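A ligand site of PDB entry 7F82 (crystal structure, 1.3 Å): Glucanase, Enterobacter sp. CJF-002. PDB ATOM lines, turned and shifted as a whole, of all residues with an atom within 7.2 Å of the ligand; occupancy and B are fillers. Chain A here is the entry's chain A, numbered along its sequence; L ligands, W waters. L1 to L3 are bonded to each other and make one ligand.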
ATOM      1  N   SER A  20      -3.106 -25.375  15.766  1.00  0.00           N
ATOM      2  CA  SER A  20      -3.099 -25.650  14.336  1.00  0.00           C
ATOM      3  C   SER A  20      -2.499 -27.026  14.095  1.00  0.00           C
ATOM      4  O   SER A  20      -1.790 -27.588  14.936  1.00  0.00           O
ATOM      5  CB  SER A  20      -2.268 -24.593  13.630  1.00  0.00           C
ATOM      6  OG  SER A  20      -0.884 -24.826  13.864  1.00  0.00           O
ATOM      7  N   GLY A  22      -0.003 -27.640  12.387  1.00  0.00           N
ATOM      8  CA  GLY A  22       1.445 -27.462  12.481  1.00  0.00           C
ATOM      9  C   GLY A  22       2.007 -27.253  13.882  1.00  0.00           C
ATOM     10  O   GLY A  22       3.226 -27.146  14.034  1.00  0.00           O
ATOM     11  N   GLY A  23       1.143 -27.129  14.895  1.00  0.00           N
ATOM     12  CA  GLY A  23       1.590 -27.064  16.271  1.00  0.00           C
ATOM     13  C   GLY A  23       1.595 -25.700  16.935  1.00  0.00           C
ATOM     14  O   GLY A  23       2.281 -25.533  17.960  1.00  0.00           O
ATOM     15  N   ARG A  24       0.863 -24.711  16.403  1.00  0.00           N
ATOM     16  CA  ARG A  24       0.820 -23.384  16.995  1.00  0.00           C
ATOM     17  C   ARG A  24      -0.518 -23.173  17.684  1.00  0.00           C
ATOM     18  O   ARG A  24      -1.574 -23.479  17.142  1.00  0.00           O
ATOM     19  CB  ARG A  24       1.176 -22.287  15.957  1.00  0.00           C
ATOM     20  CG  ARG A  24       0.005 -21.679  15.182  1.00  0.00           C
ATOM     21  CD  ARG A  24       0.478 -20.618  14.144  1.00  0.00           C
ATOM     22  NE  ARG A  24      -0.600 -19.982  13.413  1.00  0.00           N
ATOM     23  CZ  ARG A  24      -1.158 -18.812  13.748  1.00  0.00           C
ATOM     24  NH1 ARG A  24      -0.766 -18.144  14.851  1.00  0.00           N
ATOM     25  NH2 ARG A  24      -2.116 -18.287  13.003  1.00  0.00           N
ATOM     26  N   ILE A  26      -3.354 -20.826  18.667  1.00  0.00           N
ATOM     27  CA  ILE A  26      -3.864 -19.599  18.062  1.00  0.00           C
ATOM     28  C   ILE A  26      -4.863 -18.925  18.979  1.00  0.00           C
ATOM     29  O   ILE A  26      -5.821 -19.556  19.418  1.00  0.00           O
ATOM     30  CB  ILE A  26      -4.528 -19.919  16.699  1.00  0.00           C
ATOM     31  CG1 ILE A  26      -3.488 -20.604  15.778  1.00  0.00           C
ATOM     32  CG2 ILE A  26      -5.075 -18.629  16.058  1.00  0.00           C
ATOM     33  CD1 ILE A  26      -4.076 -21.055  14.376  1.00  0.00           C
ATOM     34  N   LYS A  33      -4.576 -13.265  14.410  1.00  0.00           N
ATOM     35  CA  LYS A  33      -4.593 -14.723  14.696  1.00  0.00           C
ATOM     36  C   LYS A  33      -3.242 -15.176  15.260  1.00  0.00           C
ATOM     37  O   LYS A  33      -2.518 -16.025  14.712  1.00  0.00           O
ATOM     38  CB  LYS A  33      -5.016 -15.562  13.483  1.00  0.00           C
ATOM     39  CG  LYS A  33      -6.407 -15.178  12.968  1.00  0.00           C
ATOM     40  CD  LYS A  33      -7.491 -15.395  14.019  1.00  0.00           C
ATOM     41  CE  LYS A  33      -8.843 -14.900  13.454  1.00  0.00           C
ATOM     42  NZ  LYS A  33      -9.986 -15.266  14.302  1.00  0.00           N
ATOM     43  N   THR A  35       0.017 -16.281  17.699  1.00  0.00           N
ATOM     44  CA  THR A  35       0.591 -17.229  18.652  1.00  0.00           C
ATOM     45  C   THR A  35       1.513 -16.457  19.570  1.00  0.00           C
ATOM     46  O   THR A  35       2.251 -15.561  19.114  1.00  0.00           O
ATOM     47  CB  THR A  35       1.342 -18.343  17.922  1.00  0.00           C
ATOM     48  OG1 THR A  35       0.405 -19.147  17.206  1.00  0.00           O
ATOM     49  CG2 THR A  35       2.079 -19.212  18.892  1.00  0.00           C
ATOM     50  N   GLU A  61       8.350 -28.261  18.143  1.00  0.00           N
ATOM     51  CA  GLU A  61       8.986 -27.997  16.859  1.00  0.00           C
ATOM     52  C   GLU A  61       8.481 -26.684  16.275  1.00  0.00           C
ATOM     53  O   GLU A  61       9.261 -25.927  15.692  1.00  0.00           O
ATOM     54  CB  GLU A  61       8.706 -29.155  15.888  1.00  0.00           C
ATOM     55  CG  GLU A  61       9.412 -30.446  16.268  1.00  0.00           C
ATOM     56  CD  GLU A  61      10.891 -30.262  16.475  1.00  0.00           C
ATOM     57  OE1 GLU A  61      11.526 -29.703  15.552  1.00  0.00           O
ATOM     58  OE2 GLU A  61      11.411 -30.668  17.545  1.00  0.00           O
ATOM     59  N   TRP A  62       7.170 -26.408  16.399  1.00  0.00           N
ATOM     60  CA  TRP A  62       6.702 -25.121  15.888  1.00  0.00           C
ATOM     61  C   TRP A  62       7.389 -23.955  16.600  1.00  0.00           C
ATOM     62  O   TRP A  62       7.816 -22.968  15.970  1.00  0.00           O
ATOM     63  CB  TRP A  62       5.169 -24.989  16.030  1.00  0.00           C
ATOM     64  CG  TRP A  62       4.672 -23.824  15.232  1.00  0.00           C
ATOM     65  CD1 TRP A  62       4.184 -23.893  13.948  1.00  0.00           C
ATOM     66  CD2 TRP A  62       4.671 -22.443  15.599  1.00  0.00           C
ATOM     67  NE1 TRP A  62       3.839 -22.633  13.514  1.00  0.00           N
ATOM     68  CE2 TRP A  62       4.158 -21.717  14.497  1.00  0.00           C
ATOM     69  CE3 TRP A  62       5.009 -21.741  16.784  1.00  0.00           C
ATOM     70  CZ2 TRP A  62       3.998 -20.335  14.503  1.00  0.00           C
ATOM     71  CZ3 TRP A  62       4.835 -20.347  16.806  1.00  0.00           C
ATOM     72  CH2 TRP A  62       4.325 -19.660  15.680  1.00  0.00           C
ATOM     73  N   LYS A  64      10.309 -23.915  18.210  1.00  0.00           N
ATOM     74  CA  LYS A  64      11.709 -23.814  17.806  1.00  0.00           C
ATOM     75  C   LYS A  64      11.810 -23.064  16.487  1.00  0.00           C
ATOM     76  O   LYS A  64      12.599 -22.106  16.353  1.00  0.00           O
ATOM     77  CB  LYS A  64      12.265 -25.226  17.585  1.00  0.00           C
ATOM     78  CG  LYS A  64      12.534 -26.040  18.857  1.00  0.00           C
ATOM     79  CD  LYS A  64      12.752 -27.454  18.433  1.00  0.00           C
ATOM     80  CE  LYS A  64      13.620 -28.281  19.325  1.00  0.00           C
ATOM     81  NZ  LYS A  64      14.247 -29.342  18.447  1.00  0.00           N
ATOM     82  N   ASP A  65      11.059 -23.517  15.484  1.00  0.00           N
ATOM     83  CA  ASP A  65      11.298 -23.043  14.129  1.00  0.00           C
ATOM     84  C   ASP A  65      10.774 -21.637  13.895  1.00  0.00           C
ATOM     85  O   ASP A  65      11.382 -20.864  13.137  1.00  0.00           O
ATOM     86  CB  ASP A  65      10.698 -24.014  13.136  1.00  0.00           C
ATOM     87  CG  ASP A  65      11.518 -25.295  13.054  1.00  0.00           C
ATOM     88  OD1 ASP A  65      12.666 -25.261  13.533  1.00  0.00           O
ATOM     89  OD2 ASP A  65      10.981 -26.315  12.561  1.00  0.00           O
ATOM     90  N   ASN A  66       9.666 -21.282  14.553  1.00  0.00           N
ATOM     91  CA  ASN A  66       8.994 -20.038  14.234  1.00  0.00           C
ATOM     92  C   ASN A  66       9.264 -18.929  15.233  1.00  0.00           C
ATOM     93  O   ASN A  66       9.149 -17.759  14.866  1.00  0.00           O
ATOM     94  CB  ASN A  66       7.484 -20.252  14.067  1.00  0.00           C
ATOM     95  CG  ASN A  66       7.195 -21.102  12.875  1.00  0.00           C
ATOM     96  OD1 ASN A  66       7.244 -20.617  11.739  1.00  0.00           O
ATOM     97  ND2 ASN A  66       6.986 -22.406  13.103  1.00  0.00           N
ATOM     98  N   GLN A  69      14.258 -19.225  15.852  1.00  0.00           N
ATOM     99  CA  GLN A  69      15.267 -19.342  14.781  1.00  0.00           C
ATOM    100  C   GLN A  69      15.856 -20.747  14.717  1.00  0.00           C
ATOM    101  O   GLN A  69      17.013 -20.917  14.335  1.00  0.00           O
ATOM    102  CB  GLN A  69      16.340 -18.259  14.870  1.00  0.00           C
ATOM    103  CG  GLN A  69      15.751 -16.862  14.801  1.00  0.00           C
ATOM    104  CD  GLN A  69      16.750 -15.822  15.270  1.00  0.00           C
ATOM    105  OE1 GLN A  69      16.448 -14.944  16.075  1.00  0.00           O
ATOM    106  NE2 GLN A  69      17.964 -15.942  14.780  1.00  0.00           N
ATOM    107  N   GLY A  70      15.057 -21.730  15.083  1.00  0.00           N
ATOM    108  CA  GLY A  70      15.441 -23.126  15.113  1.00  0.00           C
ATOM    109  C   GLY A  70      15.938 -23.668  16.432  1.00  0.00           C
ATOM    110  O   GLY A  70      16.049 -24.889  16.575  1.00  0.00           O
ATOM    111  N   TRP A  81       3.769 -13.764  17.419  1.00  0.00           N
ATOM    112  CA  TRP A  81       3.819 -14.196  16.021  1.00  0.00           C
ATOM    113  C   TRP A  81       2.424 -14.160  15.416  1.00  0.00           C
ATOM    114  O   TRP A  81       1.441 -14.415  16.101  1.00  0.00           O
ATOM    115  CB  TRP A  81       4.398 -15.633  15.986  1.00  0.00           C
ATOM    116  CG  TRP A  81       4.757 -16.227  14.619  1.00  0.00           C
ATOM    117  CD1 TRP A  81       6.030 -16.359  14.103  1.00  0.00           C
ATOM    118  CD2 TRP A  81       3.869 -16.812  13.665  1.00  0.00           C
ATOM    119  NE1 TRP A  81       5.961 -16.946  12.881  1.00  0.00           N
ATOM    120  CE2 TRP A  81       4.656 -17.265  12.595  1.00  0.00           C
ATOM    121  CE3 TRP A  81       2.482 -17.029  13.617  1.00  0.00           C
ATOM    122  CZ2 TRP A  81       4.098 -17.874  11.455  1.00  0.00           C
ATOM    123  CZ3 TRP A  81       1.948 -17.649  12.496  1.00  0.00           C
ATOM    124  CH2 TRP A  81       2.746 -18.075  11.434  1.00  0.00           C
ATOM    125  N   GLY A  82       2.310 -13.799  14.139  1.00  0.00           N
ATOM    126  CA  GLY A  82       0.979 -13.773  13.530  1.00  0.00           C
ATOM    127  C   GLY A  82       0.997 -13.055  12.192  1.00  0.00           C
ATOM    128  O   GLY A  82       2.038 -12.932  11.561  1.00  0.00           O
ATOM    129  N   GLU A  86      -1.090  -8.905   4.756  1.00  0.00           N
ATOM    130  CA  GLU A  86      -1.880  -9.950   4.099  1.00  0.00           C
ATOM    131  C   GLU A  86      -1.041 -11.047   3.452  1.00  0.00           C
ATOM    132  O   GLU A  86      -1.553 -12.149   3.237  1.00  0.00           O
ATOM    133  CB  GLU A  86      -2.948  -9.367   3.146  1.00  0.00           C
ATOM    134  CG  GLU A  86      -4.064  -8.568   3.885  1.00  0.00           C
ATOM    135  CD  GLU A  86      -4.900  -9.436   4.851  1.00  0.00           C
ATOM    136  OE1 GLU A  86      -5.578 -10.371   4.377  1.00  0.00           O
ATOM    137  OE2 GLU A  86      -4.884  -9.201   6.087  1.00  0.00           O
ATOM    138  N   ASN A  87       0.233 -10.788   3.175  1.00  0.00           N
ATOM    139  CA  ASN A  87       1.070 -11.819   2.572  1.00  0.00           C
ATOM    140  C   ASN A  87       2.238 -12.234   3.467  1.00  0.00           C
ATOM    141  O   ASN A  87       3.203 -12.809   2.976  1.00  0.00           O
ATOM    142  CB  ASN A  87       1.607 -11.342   1.211  1.00  0.00           C
ATOM    143  CG  ASN A  87       0.493 -10.942   0.267  1.00  0.00           C
ATOM    144  OD1 ASN A  87       0.390  -9.784  -0.161  1.00  0.00           O
ATOM    145  ND2 ASN A  87      -0.379 -11.894  -0.053  1.00  0.00           N
ATOM    146  N   ASN A  88       2.155 -11.980   4.769  1.00  0.00           N
ATOM    147  CA  ASN A  88       3.304 -12.172   5.641  1.00  0.00           C
ATOM    148  C   ASN A  88       2.880 -12.589   7.052  1.00  0.00           C
ATOM    149  O   ASN A  88       2.463 -11.736   7.823  1.00  0.00           O
ATOM    150  CB  ASN A  88       4.088 -10.869   5.680  1.00  0.00           C
ATOM    151  CG  ASN A  88       5.397 -11.002   6.326  1.00  0.00           C
ATOM    152  OD1 ASN A  88       5.923 -12.100   6.490  1.00  0.00           O
ATOM    153  ND2 ASN A  88       5.966  -9.864   6.718  1.00  0.00           N
ATOM    154  N   TRP A  89       2.989 -13.876   7.370  1.00  0.00           N
ATOM    155  CA  TRP A  89       2.800 -14.394   8.728  1.00  0.00           C
ATOM    156  C   TRP A  89       4.183 -14.643   9.316  1.00  0.00           C
ATOM    157  O   TRP A  89       4.970 -15.419   8.762  1.00  0.00           O
ATOM    158  CB  TRP A  89       1.992 -15.680   8.679  1.00  0.00           C
ATOM    159  CG  TRP A  89       0.582 -15.501   8.222  1.00  0.00           C
ATOM    160  CD1 TRP A  89       0.156 -15.331   6.932  1.00  0.00           C
ATOM    161  CD2 TRP A  89      -0.574 -15.496   9.032  1.00  0.00           C
ATOM    162  NE1 TRP A  89      -1.195 -15.195   6.892  1.00  0.00           N
ATOM    163  CE2 TRP A  89      -1.691 -15.311   8.176  1.00  0.00           C
ATOM    164  CE3 TRP A  89      -0.788 -15.641  10.396  1.00  0.00           C
ATOM    165  CZ2 TRP A  89      -2.990 -15.282   8.646  1.00  0.00           C
ATOM    166  CZ3 TRP A  89      -2.063 -15.597  10.859  1.00  0.00           C
ATOM    167  CH2 TRP A  89      -3.157 -15.408  10.002  1.00  0.00           C
ATOM    168  N   THR A  90       4.512 -13.971  10.414  1.00  0.00           N
ATOM    169  CA  THR A  90       5.904 -13.923  10.857  1.00  0.00           C
ATOM    170  C   THR A  90       5.941 -13.410  12.303  1.00  0.00           C
ATOM    171  O   THR A  90       4.906 -13.120  12.919  1.00  0.00           O
ATOM    172  CB  THR A  90       6.751 -13.070   9.899  1.00  0.00           C
ATOM    173  OG1 THR A  90       8.133 -13.258  10.211  1.00  0.00           O
ATOM    174  CG2 THR A  90       6.408 -11.584  10.014  1.00  0.00           C
HETATM  175  C1  LIG L   1      -1.579 -20.289   9.540  1.00  0.00           C
HETATM  176  C2  LIG L   1      -0.182 -19.818   9.559  1.00  0.00           C
HETATM  177  C3  LIG L   1       0.346 -19.600   8.148  1.00  0.00           C
HETATM  178  C4  LIG L   1      -0.638 -18.748   7.355  1.00  0.00           C
HETATM  179  C5  LIG L   1      -0.180 -18.647   5.883  1.00  0.00           C
HETATM  180  C6  LIG L   1      -2.465 -19.325   8.812  1.00  0.00           C
HETATM  181  O1  LIG L   1      -3.753 -19.747   8.733  1.00  0.00           O
HETATM  182  O2  LIG L   1      -2.021 -20.452  10.910  1.00  0.00           O
HETATM  183  O3  LIG L   1       0.573 -20.874  10.233  1.00  0.00           O
HETATM  184  O4  LIG L   1       1.631 -18.909   8.144  1.00  0.00           O
HETATM  185  O5  LIG L   1      -1.994 -19.278   7.394  1.00  0.00           O
HETATM  186  O6  LIG L   1      -0.215 -19.884   5.285  1.00  0.00           O
HETATM  187  C1  LG2 L   2       3.861 -18.894   7.314  1.00  0.00           C
HETATM  188  C2  LG2 L   2       5.047 -19.780   7.143  1.00  0.00           C
HETATM  189  C3  LG2 L   2       5.437 -20.559   8.364  1.00  0.00           C
HETATM  190  C4  LG2 L   2       4.231 -21.319   8.881  1.00  0.00           C
HETATM  191  C5  LG2 L   2       4.380 -21.914  10.257  1.00  0.00           C
HETATM  192  C6  LG2 L   2       2.682 -19.705   7.781  1.00  0.00           C
HETATM  193  O1  LG2 L   2       3.491 -18.304   6.028  1.00  0.00           O
HETATM  194  O2  LG2 L   2       6.190 -18.963   6.684  1.00  0.00           O
HETATM  195  O3  LG2 L   2       6.402 -21.585   7.910  1.00  0.00           O
HETATM  196  O4  LG2 L   2       3.101 -20.390   9.006  1.00  0.00           O
HETATM  197  O5  LG2 L   2       3.094 -22.328  10.783  1.00  0.00           O
HETATM  198  C1  LG3 L   3       8.263 -22.962   8.412  1.00  0.00           C
HETATM  199  C2  LG3 L   3       9.480 -23.089   9.237  1.00  0.00           C
HETATM  200  C3  LG3 L   3      10.401 -21.893   9.053  1.00  0.00           C
HETATM  201  C4  LG3 L   3       9.662 -20.578   9.348  1.00  0.00           C
HETATM  202  C5  LG3 L   3      10.599 -19.398   9.069  1.00  0.00           C
HETATM  203  C6  LG3 L   3       7.535 -21.666   8.707  1.00  0.00           C
HETATM  204  O1  LG3 L   3       7.375 -24.062   8.693  1.00  0.00           O
HETATM  205  O2  LG3 L   3      10.190 -24.300   8.848  1.00  0.00           O
HETATM  206  O3  LG3 L   3      11.495 -22.066   9.936  1.00  0.00           O
HETATM  207  O4  LG3 L   3       8.468 -20.459   8.505  1.00  0.00           O
HETATM  208  O5  LG3 L   3      10.892 -19.425   7.712  1.00  0.00           O
HETATM  209  O   HOH W   1       6.936 -17.084   8.706  1.00  0.00           O
HETATM  210  O   HOH W   2       0.269 -23.535  11.734  1.00  0.00           O
HETATM  211  O   HOH W   3       3.691 -15.762   5.363  1.00  0.00           O
HETATM  212  O   HOH W   4       6.656 -24.604  11.202  1.00  0.00           O
HETATM  213  O   HOH W   5      -5.348 -18.309  11.192  1.00  0.00           O
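O of Trp 62 sits at hydrogen-bond distance from ND2 of Asn 66, at 3.0 Å.
N of Arg 24 is in hydrogen-bond range of OG of Ser 20 (3.1 Å).
The backbone carbonyl oxygen (O) of Lys 33 sits at hydrogen-bond distance from the guanidinium group (NH1) of Arg 24.
NH1 of Arg 24 is in hydrogen-bond range of OG1 of Thr 35 (2.8 Å).
The backbone carbonyl oxygen of Trp 81 lies within hydrogen-bond range of the backbone NH of Thr 35 (2.8 Å).
NE1 of Trp 62 lies within hydrogen-bond range of O5 of LG2 L2, 2.8 Å away.
An oxygen (O2) of LIG L1 is in hydrogen-bond range of the guanidinium group (NE) of Arg 24 (2.9 Å).
The side-chain amide oxygen (OD1) of Asn 66 sits close to an oxygen (O4) of LG3 L3.
The backbone carbonyl oxygen of Asp 65 sits at hydrogen-bond distance from an oxygen (O3) of LG3 L3 (3.4 Å).
CH2 of Trp 81 touches O4 of LG2 L2, at 3.4 Å.
CB of Trp 89 touches O4 of LIG L1, 3.3 Å away.
Hydrophobic or aromatic side chains that line the ligand: Trp 62, Trp 81 and Trp 89.
The nearest printed residue that does not touch the ligand is Ile 26 (4.1 Å).
Water W3 lies within hydrogen-bond range of O1 of LG2 L2 (2.6 Å) and N of Trp 89 (2.8 Å).
Water W4 bridges an oxygen (O1) of LG3 L3 and the side-chain amide nitrogen of Asn 66.
Water W1 lies within hydrogen-bond range of O of Trp 89 (2.6 Å) and O2 of LG2 L2 (2.9 Å).
Water W2 bridges OG of Ser 20 (2.7 Å) and O3 of LIG L1 (3.1 Å).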
